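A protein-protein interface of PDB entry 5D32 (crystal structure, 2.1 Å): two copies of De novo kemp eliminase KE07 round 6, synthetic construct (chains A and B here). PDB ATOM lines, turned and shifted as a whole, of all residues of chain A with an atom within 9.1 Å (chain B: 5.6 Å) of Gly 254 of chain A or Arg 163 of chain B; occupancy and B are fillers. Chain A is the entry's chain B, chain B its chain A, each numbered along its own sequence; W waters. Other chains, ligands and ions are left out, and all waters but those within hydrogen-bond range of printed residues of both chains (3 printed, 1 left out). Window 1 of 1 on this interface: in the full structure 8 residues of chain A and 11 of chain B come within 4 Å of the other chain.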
ATOM      1  N   PHE A  38      -7.446   1.707 -11.608  1.00  0.00           N
ATOM      2  CA  PHE A  38      -8.044   2.115 -10.352  1.00  0.00           C
ATOM      3  C   PHE A  38      -8.700   0.930  -9.647  1.00  0.00           C
ATOM      4  O   PHE A  38      -8.411   0.662  -8.481  1.00  0.00           O
ATOM      5  CB  PHE A  38      -9.057   3.225 -10.564  1.00  0.00           C
ATOM      6  CG  PHE A  38      -9.684   3.697  -9.301  1.00  0.00           C
ATOM      7  CD1 PHE A  38      -8.899   4.217  -8.275  1.00  0.00           C
ATOM      8  CD2 PHE A  38     -11.051   3.612  -9.120  1.00  0.00           C
ATOM      9  CE1 PHE A  38      -9.469   4.637  -7.097  1.00  0.00           C
ATOM     10  CE2 PHE A  38     -11.625   4.045  -7.945  1.00  0.00           C
ATOM     11  CZ  PHE A  38     -10.838   4.556  -6.932  1.00  0.00           C
ATOM     12  N   TYR A  39      -9.572   0.218 -10.358  1.00  0.00           N
ATOM     13  CA  TYR A  39     -10.274  -0.927  -9.783  1.00  0.00           C
ATOM     14  C   TYR A  39      -9.310  -1.963  -9.200  1.00  0.00           C
ATOM     15  O   TYR A  39      -9.582  -2.570  -8.162  1.00  0.00           O
ATOM     16  CB  TYR A  39     -11.159  -1.583 -10.838  1.00  0.00           C
ATOM     17  CG  TYR A  39     -12.503  -0.918 -11.044  1.00  0.00           C
ATOM     18  CD1 TYR A  39     -13.316  -0.606  -9.962  1.00  0.00           C
ATOM     19  CD2 TYR A  39     -12.973  -0.631 -12.326  1.00  0.00           C
ATOM     20  CE1 TYR A  39     -14.552  -0.003 -10.138  1.00  0.00           C
ATOM     21  CE2 TYR A  39     -14.226  -0.038 -12.518  1.00  0.00           C
ATOM     22  CZ  TYR A  39     -15.007   0.270 -11.416  1.00  0.00           C
ATOM     23  OH  TYR A  39     -16.239   0.859 -11.577  1.00  0.00           O
ATOM     24  N   SER A  40      -8.180  -2.155  -9.871  1.00  0.00           N
ATOM     25  CA  SER A  40      -7.184  -3.120  -9.440  1.00  0.00           C
ATOM     26  C   SER A  40      -6.544  -2.669  -8.139  1.00  0.00           C
ATOM     27  O   SER A  40      -6.045  -3.479  -7.374  1.00  0.00           O
ATOM     28  CB  SER A  40      -6.107  -3.310 -10.511  1.00  0.00           C
ATOM     29  OG  SER A  40      -5.256  -2.179 -10.567  1.00  0.00           O
ATOM     30  N   GLU A  41      -6.567  -1.368  -7.880  1.00  0.00           N
ATOM     31  CA  GLU A  41      -5.917  -0.830  -6.692  1.00  0.00           C
ATOM     32  C   GLU A  41      -6.907  -0.540  -5.565  1.00  0.00           C
ATOM     33  O   GLU A  41      -6.546   0.090  -4.571  1.00  0.00           O
ATOM     34  CB  GLU A  41      -5.128   0.440  -7.054  1.00  0.00           C
ATOM     35  CG  GLU A  41      -3.868   0.162  -7.884  1.00  0.00           C
ATOM     36  CD  GLU A  41      -3.246   1.421  -8.459  1.00  0.00           C
ATOM     37  OE1 GLU A  41      -3.999   2.373  -8.770  1.00  0.00           O
ATOM     38  OE2 GLU A  41      -2.003   1.463  -8.595  1.00  0.00           O
ATOM     39  N   ILE A  42      -8.152  -1.000  -5.700  1.00  0.00           N
ATOM     40  CA  ILE A  42      -9.103  -0.832  -4.597  1.00  0.00           C
ATOM     41  C   ILE A  42      -9.884  -2.083  -4.200  1.00  0.00           C
ATOM     42  O   ILE A  42     -10.711  -2.021  -3.285  1.00  0.00           O
ATOM     43  CB  ILE A  42     -10.140   0.266  -4.891  1.00  0.00           C
ATOM     44  CG1 ILE A  42     -11.057  -0.136  -6.042  1.00  0.00           C
ATOM     45  CG2 ILE A  42      -9.467   1.578  -5.173  1.00  0.00           C
ATOM     46  CD1 ILE A  42     -12.254   0.801  -6.191  1.00  0.00           C
ATOM     47  N   GLY A  43      -9.653  -3.207  -4.873  1.00  0.00           N
ATOM     48  CA  GLY A  43     -10.278  -4.446  -4.435  1.00  0.00           C
ATOM     49  C   GLY A  43     -10.844  -5.376  -5.497  1.00  0.00           C
ATOM     50  O   GLY A  43     -11.254  -6.504  -5.187  1.00  0.00           O
ATOM     51  N   ILE A  44     -10.887  -4.929  -6.748  1.00  0.00           N
ATOM     52  CA  ILE A  44     -11.371  -5.809  -7.802  1.00  0.00           C
ATOM     53  C   ILE A  44     -10.361  -6.937  -8.003  1.00  0.00           C
ATOM     54  O   ILE A  44      -9.150  -6.707  -7.996  1.00  0.00           O
ATOM     55  CB  ILE A  44     -11.630  -5.046  -9.128  1.00  0.00           C
ATOM     56  CG1 ILE A  44     -12.866  -4.161  -8.989  1.00  0.00           C
ATOM     57  CG2 ILE A  44     -11.888  -6.009 -10.248  1.00  0.00           C
ATOM     58  CD1 ILE A  44     -14.118  -4.915  -8.559  1.00  0.00           C
ATOM     59  N   VAL A 234     -16.722  -0.970  -3.931  1.00  0.00           N
ATOM     60  CA  VAL A 234     -16.038  -2.257  -4.022  1.00  0.00           C
ATOM     61  C   VAL A 234     -15.440  -2.711  -2.696  1.00  0.00           C
ATOM     62  O   VAL A 234     -15.590  -3.874  -2.308  1.00  0.00           O
ATOM     63  CB  VAL A 234     -14.912  -2.208  -5.088  1.00  0.00           C
ATOM     64  CG1 VAL A 234     -13.992  -3.424  -4.969  1.00  0.00           C
ATOM     65  CG2 VAL A 234     -15.517  -2.074  -6.488  1.00  0.00           C
ATOM     66  N   ARG A 235     -14.743  -1.805  -2.011  1.00  0.00           N
ATOM     67  CA  ARG A 235     -14.230  -2.140  -0.703  1.00  0.00           C
ATOM     68  C   ARG A 235     -15.387  -2.464   0.241  1.00  0.00           C
ATOM     69  O   ARG A 235     -15.341  -3.462   0.968  1.00  0.00           O
ATOM     70  CB  ARG A 235     -13.388  -1.012  -0.117  1.00  0.00           C
ATOM     71  CG  ARG A 235     -12.988  -1.305   1.329  1.00  0.00           C
ATOM     72  CD  ARG A 235     -12.698  -0.034   2.110  1.00  0.00           C
ATOM     73  NE  ARG A 235     -11.275   0.196   2.260  1.00  0.00           N
ATOM     74  CZ  ARG A 235     -10.661   1.348   1.987  1.00  0.00           C
ATOM     75  NH1 ARG A 235     -11.342   2.401   1.536  1.00  0.00           N
ATOM     76  NH2 ARG A 235      -9.350   1.442   2.164  1.00  0.00           N
ATOM     77  N   LYS A 238     -16.532  -5.942  -0.537  1.00  0.00           N
ATOM     78  CA  LYS A 238     -15.628  -6.984  -0.041  1.00  0.00           C
ATOM     79  C   LYS A 238     -15.740  -7.160   1.482  1.00  0.00           C
ATOM     80  O   LYS A 238     -15.769  -8.293   1.991  1.00  0.00           O
ATOM     81  CB  LYS A 238     -14.178  -6.678  -0.428  1.00  0.00           C
ATOM     82  CG  LYS A 238     -13.838  -6.930  -1.906  1.00  0.00           C
ATOM     83  CD  LYS A 238     -13.717  -8.406  -2.207  1.00  0.00           C
ATOM     84  CE  LYS A 238     -13.056  -8.650  -3.567  1.00  0.00           C
ATOM     85  NZ  LYS A 238     -11.571  -8.503  -3.522  1.00  0.00           N
ATOM     86  N   GLU A 239     -15.815  -6.049   2.208  1.00  0.00           N
ATOM     87  CA  GLU A 239     -15.911  -6.134   3.669  1.00  0.00           C
ATOM     88  C   GLU A 239     -17.232  -6.758   4.093  1.00  0.00           C
ATOM     89  O   GLU A 239     -17.279  -7.475   5.090  1.00  0.00           O
ATOM     90  CB  GLU A 239     -15.759  -4.757   4.319  1.00  0.00           C
ATOM     91  CG  GLU A 239     -14.372  -4.166   4.194  1.00  0.00           C
ATOM     92  CD  GLU A 239     -14.304  -2.727   4.665  1.00  0.00           C
ATOM     93  OE1 GLU A 239     -15.367  -2.094   4.854  1.00  0.00           O
ATOM     94  OE2 GLU A 239     -13.185  -2.221   4.843  1.00  0.00           O
ATOM     95  N   ARG A 249     -10.901 -12.180  -1.083  1.00  0.00           N
ATOM     96  CA  ARG A 249      -9.553 -11.635  -0.980  1.00  0.00           C
ATOM     97  C   ARG A 249      -9.567 -10.149  -0.603  1.00  0.00           C
ATOM     98  O   ARG A 249     -10.212  -9.345  -1.273  1.00  0.00           O
ATOM     99  CB  ARG A 249      -8.808 -11.822  -2.293  1.00  0.00           C
ATOM    100  CG  ARG A 249      -8.563 -13.269  -2.652  1.00  0.00           C
ATOM    101  CD  ARG A 249      -7.739 -13.377  -3.913  1.00  0.00           C
ATOM    102  NE  ARG A 249      -6.368 -12.938  -3.678  1.00  0.00           N
ATOM    103  CZ  ARG A 249      -5.425 -13.696  -3.122  1.00  0.00           C
ATOM    104  NH1 ARG A 249      -5.700 -14.947  -2.747  1.00  0.00           N
ATOM    105  NH2 ARG A 249      -4.204 -13.201  -2.942  1.00  0.00           N
ATOM    106  N   LEU A 250      -8.850  -9.799   0.469  1.00  0.00           N
ATOM    107  CA  LEU A 250      -8.771  -8.411   0.961  1.00  0.00           C
ATOM    108  C   LEU A 250      -7.431  -7.732   0.671  1.00  0.00           C
ATOM    109  O   LEU A 250      -7.227  -6.586   1.059  1.00  0.00           O
ATOM    110  CB  LEU A 250      -9.019  -8.356   2.476  1.00  0.00           C
ATOM    111  CG  LEU A 250     -10.256  -9.082   2.994  1.00  0.00           C
ATOM    112  CD1 LEU A 250     -10.346  -8.997   4.512  1.00  0.00           C
ATOM    113  CD2 LEU A 250     -11.491  -8.503   2.368  1.00  0.00           C
ATOM    114  N   GLU A 251      -6.528  -8.437   0.001  1.00  0.00           N
ATOM    115  CA  GLU A 251      -5.162  -7.967  -0.237  1.00  0.00           C
ATOM    116  C   GLU A 251      -5.126  -6.667  -1.016  1.00  0.00           C
ATOM    117  O   GLU A 251      -4.248  -5.826  -0.810  1.00  0.00           O
ATOM    118  CB  GLU A 251      -4.353  -9.022  -1.005  1.00  0.00           C
ATOM    119  CG  GLU A 251      -4.079 -10.316  -0.263  1.00  0.00           C
ATOM    120  CD  GLU A 251      -5.235 -11.296  -0.338  1.00  0.00           C
ATOM    121  OE1 GLU A 251      -6.320 -10.873  -0.779  1.00  0.00           O
ATOM    122  OE2 GLU A 251      -5.060 -12.480   0.050  1.00  0.00           O
ATOM    123  N   GLY A 252      -6.089  -6.503  -1.912  1.00  0.00           N
ATOM    124  CA  GLY A 252      -6.076  -5.393  -2.840  1.00  0.00           C
ATOM    125  C   GLY A 252      -6.640  -4.136  -2.223  1.00  0.00           C
ATOM    126  O   GLY A 252      -6.421  -3.044  -2.734  1.00  0.00           O
ATOM    127  N   LEU A 253      -7.363  -4.292  -1.117  1.00  0.00           N
ATOM    128  CA  LEU A 253      -8.002  -3.155  -0.474  1.00  0.00           C
ATOM    129  C   LEU A 253      -6.951  -2.138  -0.007  1.00  0.00           C
ATOM    130  O   LEU A 253      -5.839  -2.514   0.368  1.00  0.00           O
ATOM    131  CB  LEU A 253      -8.871  -3.622   0.706  1.00  0.00           C
ATOM    132  CG  LEU A 253     -10.016  -4.625   0.464  1.00  0.00           C
ATOM    133  CD1 LEU A 253     -10.919  -4.721   1.678  1.00  0.00           C
ATOM    134  CD2 LEU A 253     -10.841  -4.259  -0.749  1.00  0.00           C
ATOM    135  N   GLY A 254      -7.301  -0.857  -0.082  1.00  0.00           N
ATOM    136  CA  GLY A 254      -6.478   0.225   0.437  1.00  0.00           C
ATOM    137  C   GLY A 254      -5.055   0.342  -0.081  1.00  0.00           C
ATOM    138  O   GLY A 254      -4.206   0.934   0.586  1.00  0.00           O
ATOM    139  N   SER A 255      -4.784  -0.204  -1.265  1.00  0.00           N
ATOM    140  CA  SER A 255      -3.438  -0.138  -1.845  1.00  0.00           C
ATOM    141  C   SER A 255      -3.001   1.279  -2.222  1.00  0.00           C
ATOM    142  O   SER A 255      -1.810   1.557  -2.348  1.00  0.00           O
ATOM    143  CB  SER A 255      -3.366  -1.027  -3.072  1.00  0.00           C
ATOM    144  OG  SER A 255      -3.979  -2.261  -2.777  1.00  0.00           O
ATOM    145  N   LEU A 256      -3.977   2.162  -2.405  1.00  0.00           N
ATOM    146  CA  LEU A 256      -3.714   3.563  -2.709  1.00  0.00           C
ATOM    147  C   LEU A 256      -3.610   4.416  -1.453  1.00  0.00           C
ATOM    148  O   LEU A 256      -3.360   5.617  -1.537  1.00  0.00           O
ATOM    149  CB  LEU A 256      -4.818   4.144  -3.605  1.00  0.00           C
ATOM    150  CG  LEU A 256      -4.986   3.589  -5.013  1.00  0.00           C
ATOM    151  CD1 LEU A 256      -5.975   4.440  -5.796  1.00  0.00           C
ATOM    152  CD2 LEU A 256      -3.648   3.510  -5.720  1.00  0.00           C
ATOM    153  N   GLU A 257      -3.822   3.823  -0.287  1.00  0.00           N
ATOM    154  CA  GLU A 257      -3.821   4.635   0.915  1.00  0.00           C
ATOM    155  C   GLU A 257      -2.510   4.494   1.670  1.00  0.00           C
ATOM    156  O   GLU A 257      -1.807   3.502   1.520  1.00  0.00           O
ATOM    157  CB  GLU A 257      -5.007   4.259   1.790  1.00  0.00           C
ATOM    158  CG  GLU A 257      -6.298   4.199   1.007  1.00  0.00           C
ATOM    159  CD  GLU A 257      -7.465   3.780   1.863  1.00  0.00           C
ATOM    160  OE1 GLU A 257      -7.240   3.019   2.823  1.00  0.00           O
ATOM    161  OE2 GLU A 257      -8.602   4.224   1.593  1.00  0.00           O
ATOM    162  N   HIS A 258      -2.195   5.489   2.492  1.00  0.00           N
ATOM    163  CA  HIS A 258      -0.915   5.530   3.178  1.00  0.00           C
ATOM    164  C   HIS A 258      -1.102   5.937   4.642  1.00  0.00           C
ATOM    165  O   HIS A 258      -2.211   6.267   5.076  1.00  0.00           O
ATOM    166  CB  HIS A 258       0.036   6.501   2.456  1.00  0.00           C
ATOM    167  CG  HIS A 258      -0.560   7.857   2.232  1.00  0.00           C
ATOM    168  ND1 HIS A 258      -0.650   8.806   3.233  1.00  0.00           N
ATOM    169  CD2 HIS A 258      -1.128   8.413   1.135  1.00  0.00           C
ATOM    170  CE1 HIS A 258      -1.232   9.890   2.755  1.00  0.00           C
ATOM    171  NE2 HIS A 258      -1.528   9.680   1.484  1.00  0.00           N
ATOM    172  N   HIS A 259      -0.010   5.903   5.403  1.00  0.00           N
ATOM    173  CA  HIS A 259      -0.080   6.098   6.842  1.00  0.00           C
ATOM    174  C   HIS A 259       0.313   7.513   7.206  1.00  0.00           C
ATOM    175  O   HIS A 259       0.448   7.850   8.380  1.00  0.00           O
ATOM    176  CB  HIS A 259       0.815   5.097   7.563  1.00  0.00           C
ATOM    177  CG  HIS A 259       2.254   5.165   7.149  1.00  0.00           C
ATOM    178  ND1 HIS A 259       2.693   4.737   5.914  1.00  0.00           N
ATOM    179  CD2 HIS A 259       3.354   5.599   7.811  1.00  0.00           C
ATOM    180  CE1 HIS A 259       4.001   4.906   5.833  1.00  0.00           C
ATOM    181  NE2 HIS A 259       4.426   5.428   6.971  1.00  0.00           N
ATOM    182  N   HIS A 260       0.497   8.334   6.181  1.00  0.00           N
ATOM    183  CA  HIS A 260       0.733   9.753   6.364  1.00  0.00           C
ATOM    184  C   HIS A 260      -0.580  10.518   6.291  1.00  0.00           C
ATOM    185  O   HIS A 260      -1.640   9.944   6.032  1.00  0.00           O
ATOM    186  CB  HIS A 260       1.723  10.254   5.317  1.00  0.00           C
ATOM    187  CG  HIS A 260       2.989   9.461   5.286  1.00  0.00           C
ATOM    188  ND1 HIS A 260       3.345   8.667   4.218  1.00  0.00           N
ATOM    189  CD2 HIS A 260       3.953   9.290   6.222  1.00  0.00           C
ATOM    190  CE1 HIS A 260       4.488   8.063   4.486  1.00  0.00           C
ATOM    191  NE2 HIS A 260       4.878   8.424   5.694  1.00  0.00           N
ATOM    192  N   PRO B 110      -3.419  -6.412   4.310  1.00  0.00           N
ATOM    193  CA  PRO B 110      -2.303  -5.474   4.489  1.00  0.00           C
ATOM    194  C   PRO B 110      -2.732  -4.080   4.934  1.00  0.00           C
ATOM    195  O   PRO B 110      -1.902  -3.338   5.436  1.00  0.00           O
ATOM    196  CB  PRO B 110      -1.667  -5.407   3.102  1.00  0.00           C
ATOM    197  CG  PRO B 110      -2.093  -6.670   2.417  1.00  0.00           C
ATOM    198  CD  PRO B 110      -3.429  -7.021   2.968  1.00  0.00           C
ATOM    199  N   SER B 111      -3.999  -3.737   4.749  1.00  0.00           N
ATOM    200  CA  SER B 111      -4.519  -2.436   5.188  1.00  0.00           C
ATOM    201  C   SER B 111      -4.365  -2.265   6.691  1.00  0.00           C
ATOM    202  O   SER B 111      -4.324  -1.154   7.199  1.00  0.00           O
ATOM    203  CB  SER B 111      -5.996  -2.293   4.817  1.00  0.00           C
ATOM    204  OG  SER B 111      -6.198  -2.529   3.436  1.00  0.00           O
ATOM    205  N   ILE B 113      -1.811  -2.948   8.502  1.00  0.00           N
ATOM    206  CA  ILE B 113      -0.549  -2.257   8.713  1.00  0.00           C
ATOM    207  C   ILE B 113      -0.745  -0.736   8.700  1.00  0.00           C
ATOM    208  O   ILE B 113      -0.327  -0.020   9.617  1.00  0.00           O
ATOM    209  CB  ILE B 113       0.482  -2.626   7.619  1.00  0.00           C
ATOM    210  CG1 ILE B 113       0.735  -4.128   7.579  1.00  0.00           C
ATOM    211  CG2 ILE B 113       1.782  -1.899   7.865  1.00  0.00           C
ATOM    212  CD1 ILE B 113       1.615  -4.564   6.407  1.00  0.00           C
ATOM    213  N   THR B 114      -1.397  -0.254   7.649  1.00  0.00           N
ATOM    214  CA  THR B 114      -1.554   1.173   7.432  1.00  0.00           C
ATOM    215  C   THR B 114      -2.451   1.834   8.468  1.00  0.00           C
ATOM    216  O   THR B 114      -2.138   2.903   8.955  1.00  0.00           O
ATOM    217  CB  THR B 114      -2.143   1.464   6.052  1.00  0.00           C
ATOM    218  OG1 THR B 114      -1.344   0.830   5.046  1.00  0.00           O
ATOM    219  CG2 THR B 114      -2.209   3.010   5.818  1.00  0.00           C
ATOM    220  N   ALA B 117      -0.487   2.164  11.749  1.00  0.00           N
ATOM    221  CA  ALA B 117       0.569   3.161  11.580  1.00  0.00           C
ATOM    222  C   ALA B 117      -0.016   4.555  11.395  1.00  0.00           C
ATOM    223  O   ALA B 117       0.592   5.549  11.782  1.00  0.00           O
ATOM    224  CB  ALA B 117       1.460   2.801  10.395  1.00  0.00           C
ATOM    225  N   VAL B 158       8.325  -5.758   0.249  1.00  0.00           N
ATOM    226  CA  VAL B 158       8.130  -4.452  -0.390  1.00  0.00           C
ATOM    227  C   VAL B 158       6.787  -3.837   0.014  1.00  0.00           C
ATOM    228  O   VAL B 158       6.708  -2.678   0.436  1.00  0.00           O
ATOM    229  CB  VAL B 158       8.206  -4.589  -1.934  1.00  0.00           C
ATOM    230  CG1 VAL B 158       7.941  -3.265  -2.614  1.00  0.00           C
ATOM    231  CG2 VAL B 158       9.565  -5.138  -2.327  1.00  0.00           C
ATOM    232  N   GLU B 159       5.735  -4.635  -0.105  1.00  0.00           N
ATOM    233  CA  GLU B 159       4.389  -4.227   0.312  1.00  0.00           C
ATOM    234  C   GLU B 159       4.327  -3.818   1.786  1.00  0.00           C
ATOM    235  O   GLU B 159       3.655  -2.856   2.155  1.00  0.00           O
ATOM    236  CB  GLU B 159       3.419  -5.368   0.057  1.00  0.00           C
ATOM    237  CG  GLU B 159       1.971  -5.027   0.291  1.00  0.00           C
ATOM    238  CD  GLU B 159       1.466  -4.034  -0.725  1.00  0.00           C
ATOM    239  OE1 GLU B 159       0.496  -3.304  -0.412  1.00  0.00           O
ATOM    240  OE2 GLU B 159       2.046  -3.985  -1.837  1.00  0.00           O
ATOM    241  N   VAL B 160       5.033  -4.554   2.633  1.00  0.00           N
ATOM    242  CA  VAL B 160       5.029  -4.281   4.069  1.00  0.00           C
ATOM    243  C   VAL B 160       5.613  -2.910   4.385  1.00  0.00           C
ATOM    244  O   VAL B 160       5.095  -2.167   5.236  1.00  0.00           O
ATOM    245  CB  VAL B 160       5.795  -5.375   4.815  1.00  0.00           C
ATOM    246  CG1 VAL B 160       6.170  -4.933   6.211  1.00  0.00           C
ATOM    247  CG2 VAL B 160       4.956  -6.638   4.847  1.00  0.00           C
ATOM    248  N   GLU B 161       6.683  -2.556   3.688  1.00  0.00           N
ATOM    249  CA  GLU B 161       7.244  -1.218   3.870  1.00  0.00           C
ATOM    250  C   GLU B 161       6.279  -0.180   3.304  1.00  0.00           C
ATOM    251  O   GLU B 161       5.956   0.809   3.958  1.00  0.00           O
ATOM    252  CB  GLU B 161       8.618  -1.083   3.202  1.00  0.00           C
ATOM    253  CG  GLU B 161       9.186   0.344   3.308  1.00  0.00           C
ATOM    254  CD  GLU B 161      10.674   0.433   2.986  1.00  0.00           C
ATOM    255  OE1 GLU B 161      11.295  -0.610   2.688  1.00  0.00           O
ATOM    256  OE2 GLU B 161      11.217   1.561   3.046  1.00  0.00           O
ATOM    257  N   LYS B 162       5.816  -0.434   2.088  1.00  0.00           N
ATOM    258  CA  LYS B 162       4.865   0.429   1.408  1.00  0.00           C
ATOM    259  C   LYS B 162       3.686   0.814   2.320  1.00  0.00           C
ATOM    260  O   LYS B 162       3.362   1.996   2.474  1.00  0.00           O
ATOM    261  CB  LYS B 162       4.379  -0.273   0.141  1.00  0.00           C
ATOM    262  CG  LYS B 162       3.366   0.483  -0.660  1.00  0.00           C
ATOM    263  CD  LYS B 162       2.978  -0.321  -1.886  1.00  0.00           C
ATOM    264  CE  LYS B 162       2.046   0.472  -2.779  1.00  0.00           C
ATOM    265  NZ  LYS B 162       1.684  -0.294  -4.015  1.00  0.00           N
ATOM    266  N   ARG B 163       3.081  -0.185   2.944  1.00  0.00           N
ATOM    267  CA  ARG B 163       1.934  -0.007   3.832  1.00  0.00           C
ATOM    268  C   ARG B 163       2.226   0.789   5.120  1.00  0.00           C
ATOM    269  O   ARG B 163       1.304   1.306   5.749  1.00  0.00           O
ATOM    270  CB  ARG B 163       1.363  -1.389   4.217  1.00  0.00           C
ATOM    271  CG  ARG B 163       0.804  -2.212   3.045  1.00  0.00           C
ATOM    272  CD  ARG B 163      -0.503  -1.631   2.468  1.00  0.00           C
ATOM    273  NE  ARG B 163      -1.102  -2.552   1.511  1.00  0.00           N
ATOM    274  CZ  ARG B 163      -2.389  -2.553   1.169  1.00  0.00           C
ATOM    275  NH1 ARG B 163      -3.226  -1.687   1.722  1.00  0.00           N
ATOM    276  NH2 ARG B 163      -2.844  -3.442   0.294  1.00  0.00           N
ATOM    277  N   GLY B 164       3.487   0.850   5.531  1.00  0.00           N
ATOM    278  CA  GLY B 164       3.861   1.610   6.714  1.00  0.00           C
ATOM    279  C   GLY B 164       4.332   0.858   7.954  1.00  0.00           C
ATOM    280  O   GLY B 164       4.247   1.376   9.061  1.00  0.00           O
ATOM    281  N   ALA B 165       4.835  -0.359   7.794  1.00  0.00           N
ATOM    282  CA  ALA B 165       5.406  -1.059   8.937  1.00  0.00           C
ATOM    283  C   ALA B 165       6.689  -0.339   9.406  1.00  0.00           C
ATOM    284  O   ALA B 165       7.317   0.382   8.630  1.00  0.00           O
ATOM    285  CB  ALA B 165       5.683  -2.475   8.589  1.00  0.00           C
HETATM  286  O   HOH W   1      -3.295   0.645   2.858  1.00  0.00           O
HETATM  287  O   HOH W   2      -9.117  -1.386   3.803  1.00  0.00           O
HETATM  288  O   HOH W   3       1.751   3.714   3.721  1.00  0.00           O
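No position is printed for both chains. Of the 11 pairs that touch across the chains among the printed residues, none has its exchanged pair printed and touching as well.
Water W1 lies within hydrogen-bond range of the backbone carbonyl oxygen (O) of Gly 254 of chain A (2.5 Å), the guanidinium group (NH1) of Arg 163 of chain B (2.6 Å), the side-chain hydroxyl (OG1) of Thr 114 of chain B (2.9 Å) and the backbone carbonyl oxygen (O) of Glu 257 of chain A (3.5 Å). Water W3 lies within hydrogen-bond range of a ring nitrogen (ND1) of His 259 of chain A (2.6 Å), the backbone carbonyl oxygen of Lys 162 of chain B (2.7 Å) and the backbone carbonyl oxygen of Arg 163 of chain B (3.2 Å). Water W2 bridges the guanidinium group (NE) of Arg 235 of chain A and the side-chain hydroxyl (OG) of Ser 111 of chain B.
Printed residues of chain B that touch a printed residue of chain A: Pro 110, Ser 111, Thr 114, Ala 117, Arg 163 and Gly 164. Printed residues of chain A that touch a printed residue of chain B: Glu 251, Leu 253, Gly 254, Ser 255, His 258 and His 259. Hydrophobic or aromatic side chains of chain A that line the printed part of chain B: Leu 253 and His 259. Along chain A the printed residues that touch a printed residue of chain B span positions 251 to 259.
O of Arg 163 of chain B lies within hydrogen-bond range of OG1 of Thr 114 of chain B. OE1 of Glu 159 of chain B is in salt-bridge range of NE of Arg 163 of chain B (2.6 Å). The guanidinium group (NH2) of Arg 249 of chain A lies within salt-bridge range of the side-chain carboxylate (OE2) of Glu 251 of chain A. The side-chain hydroxyl of Ser 255 of chain A lies within hydrogen-bond range of the backbone carbonyl oxygen of Gly 252 of chain A (2.6 Å). O of His 260 of chain A lies within hydrogen-bond range of ND1 of His 258 of chain A. A ring nitrogen (NE2) of His 260 of chain A is in hydrogen-bond range of a ring nitrogen (NE2) of His 259 of chain A (3.3 Å).
Of the printed residues of chain B, Glu 251 of chain A touches Pro 110 (3.8 Å) and Arg 163 (3.0 Å). Of the printed residues of chain B, Leu 253 of chain A touches Ser 111 (3.1 Å) and Arg 163 (3.1 Å). Of chain B, only Arg 163 (3.0 Å) comes within 4 Å of Gly 254 of chain A. Printed residues of chain B within 4 Å of Ser 255 of chain A: Arg 163. Of the printed residues of chain B, His 258 of chain A touches Thr 114 (3.3 Å). Ile 113 of chain B touches none of the printed residues of chain A. Thr 114 of chain B touches just these residues of chain A: His 258 and His 259. Lys 162 of chain B touches none of the printed residues of chain A. Of chain A, only Glu 251, Leu 253, Gly 254, Ser 255 and His 259 come within 4 Å of Arg 163 of chain B. Gly 164 of chain B touches just one residue of chain A: His 259 (3.4 Å). The nearest residue of chain A that does not touch Arg 163 of chain B is Gly 252 of chain A (4.6 Å).
Among the printed residues, pairs that only touch across the chains: Glu 251 of chain A with Pro 110 of chain B (3.8 Å), His 258 of chain A with Thr 114 of chain B (3.3 Å), His 259 of chain A with Thr 114 of chain B (3.7 Å), His 259 of chain A with Ala 117 of chain B (3.7 Å), His 259 of chain A with Arg 163 of chain B (3.7 Å) and His 259 of chain A with Gly 164 of chain B (3.4 Å).
The side-chain hydroxyl of Ser 111 of chain B lies within hydrogen-bond range of the backbone carbonyl oxygen of Leu 253 of chain A (3.1 Å). NH2 of Arg 163 of chain B sits at hydrogen-bond distance from O of Glu 251 of chain A, at 3.0 Å. The guanidinium group of Arg 163 of chain B lies within hydrogen-bond range of the backbone carbonyl oxygen of Leu 253 of chain A, at 3.1 Å. NH1 of Arg 163 of chain B is in hydrogen-bond range of O of Gly 254 of chain A (3.0 Å). NH2 of Arg 163 of chain B is in hydrogen-bond range of OG of Ser 255 of chain A.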
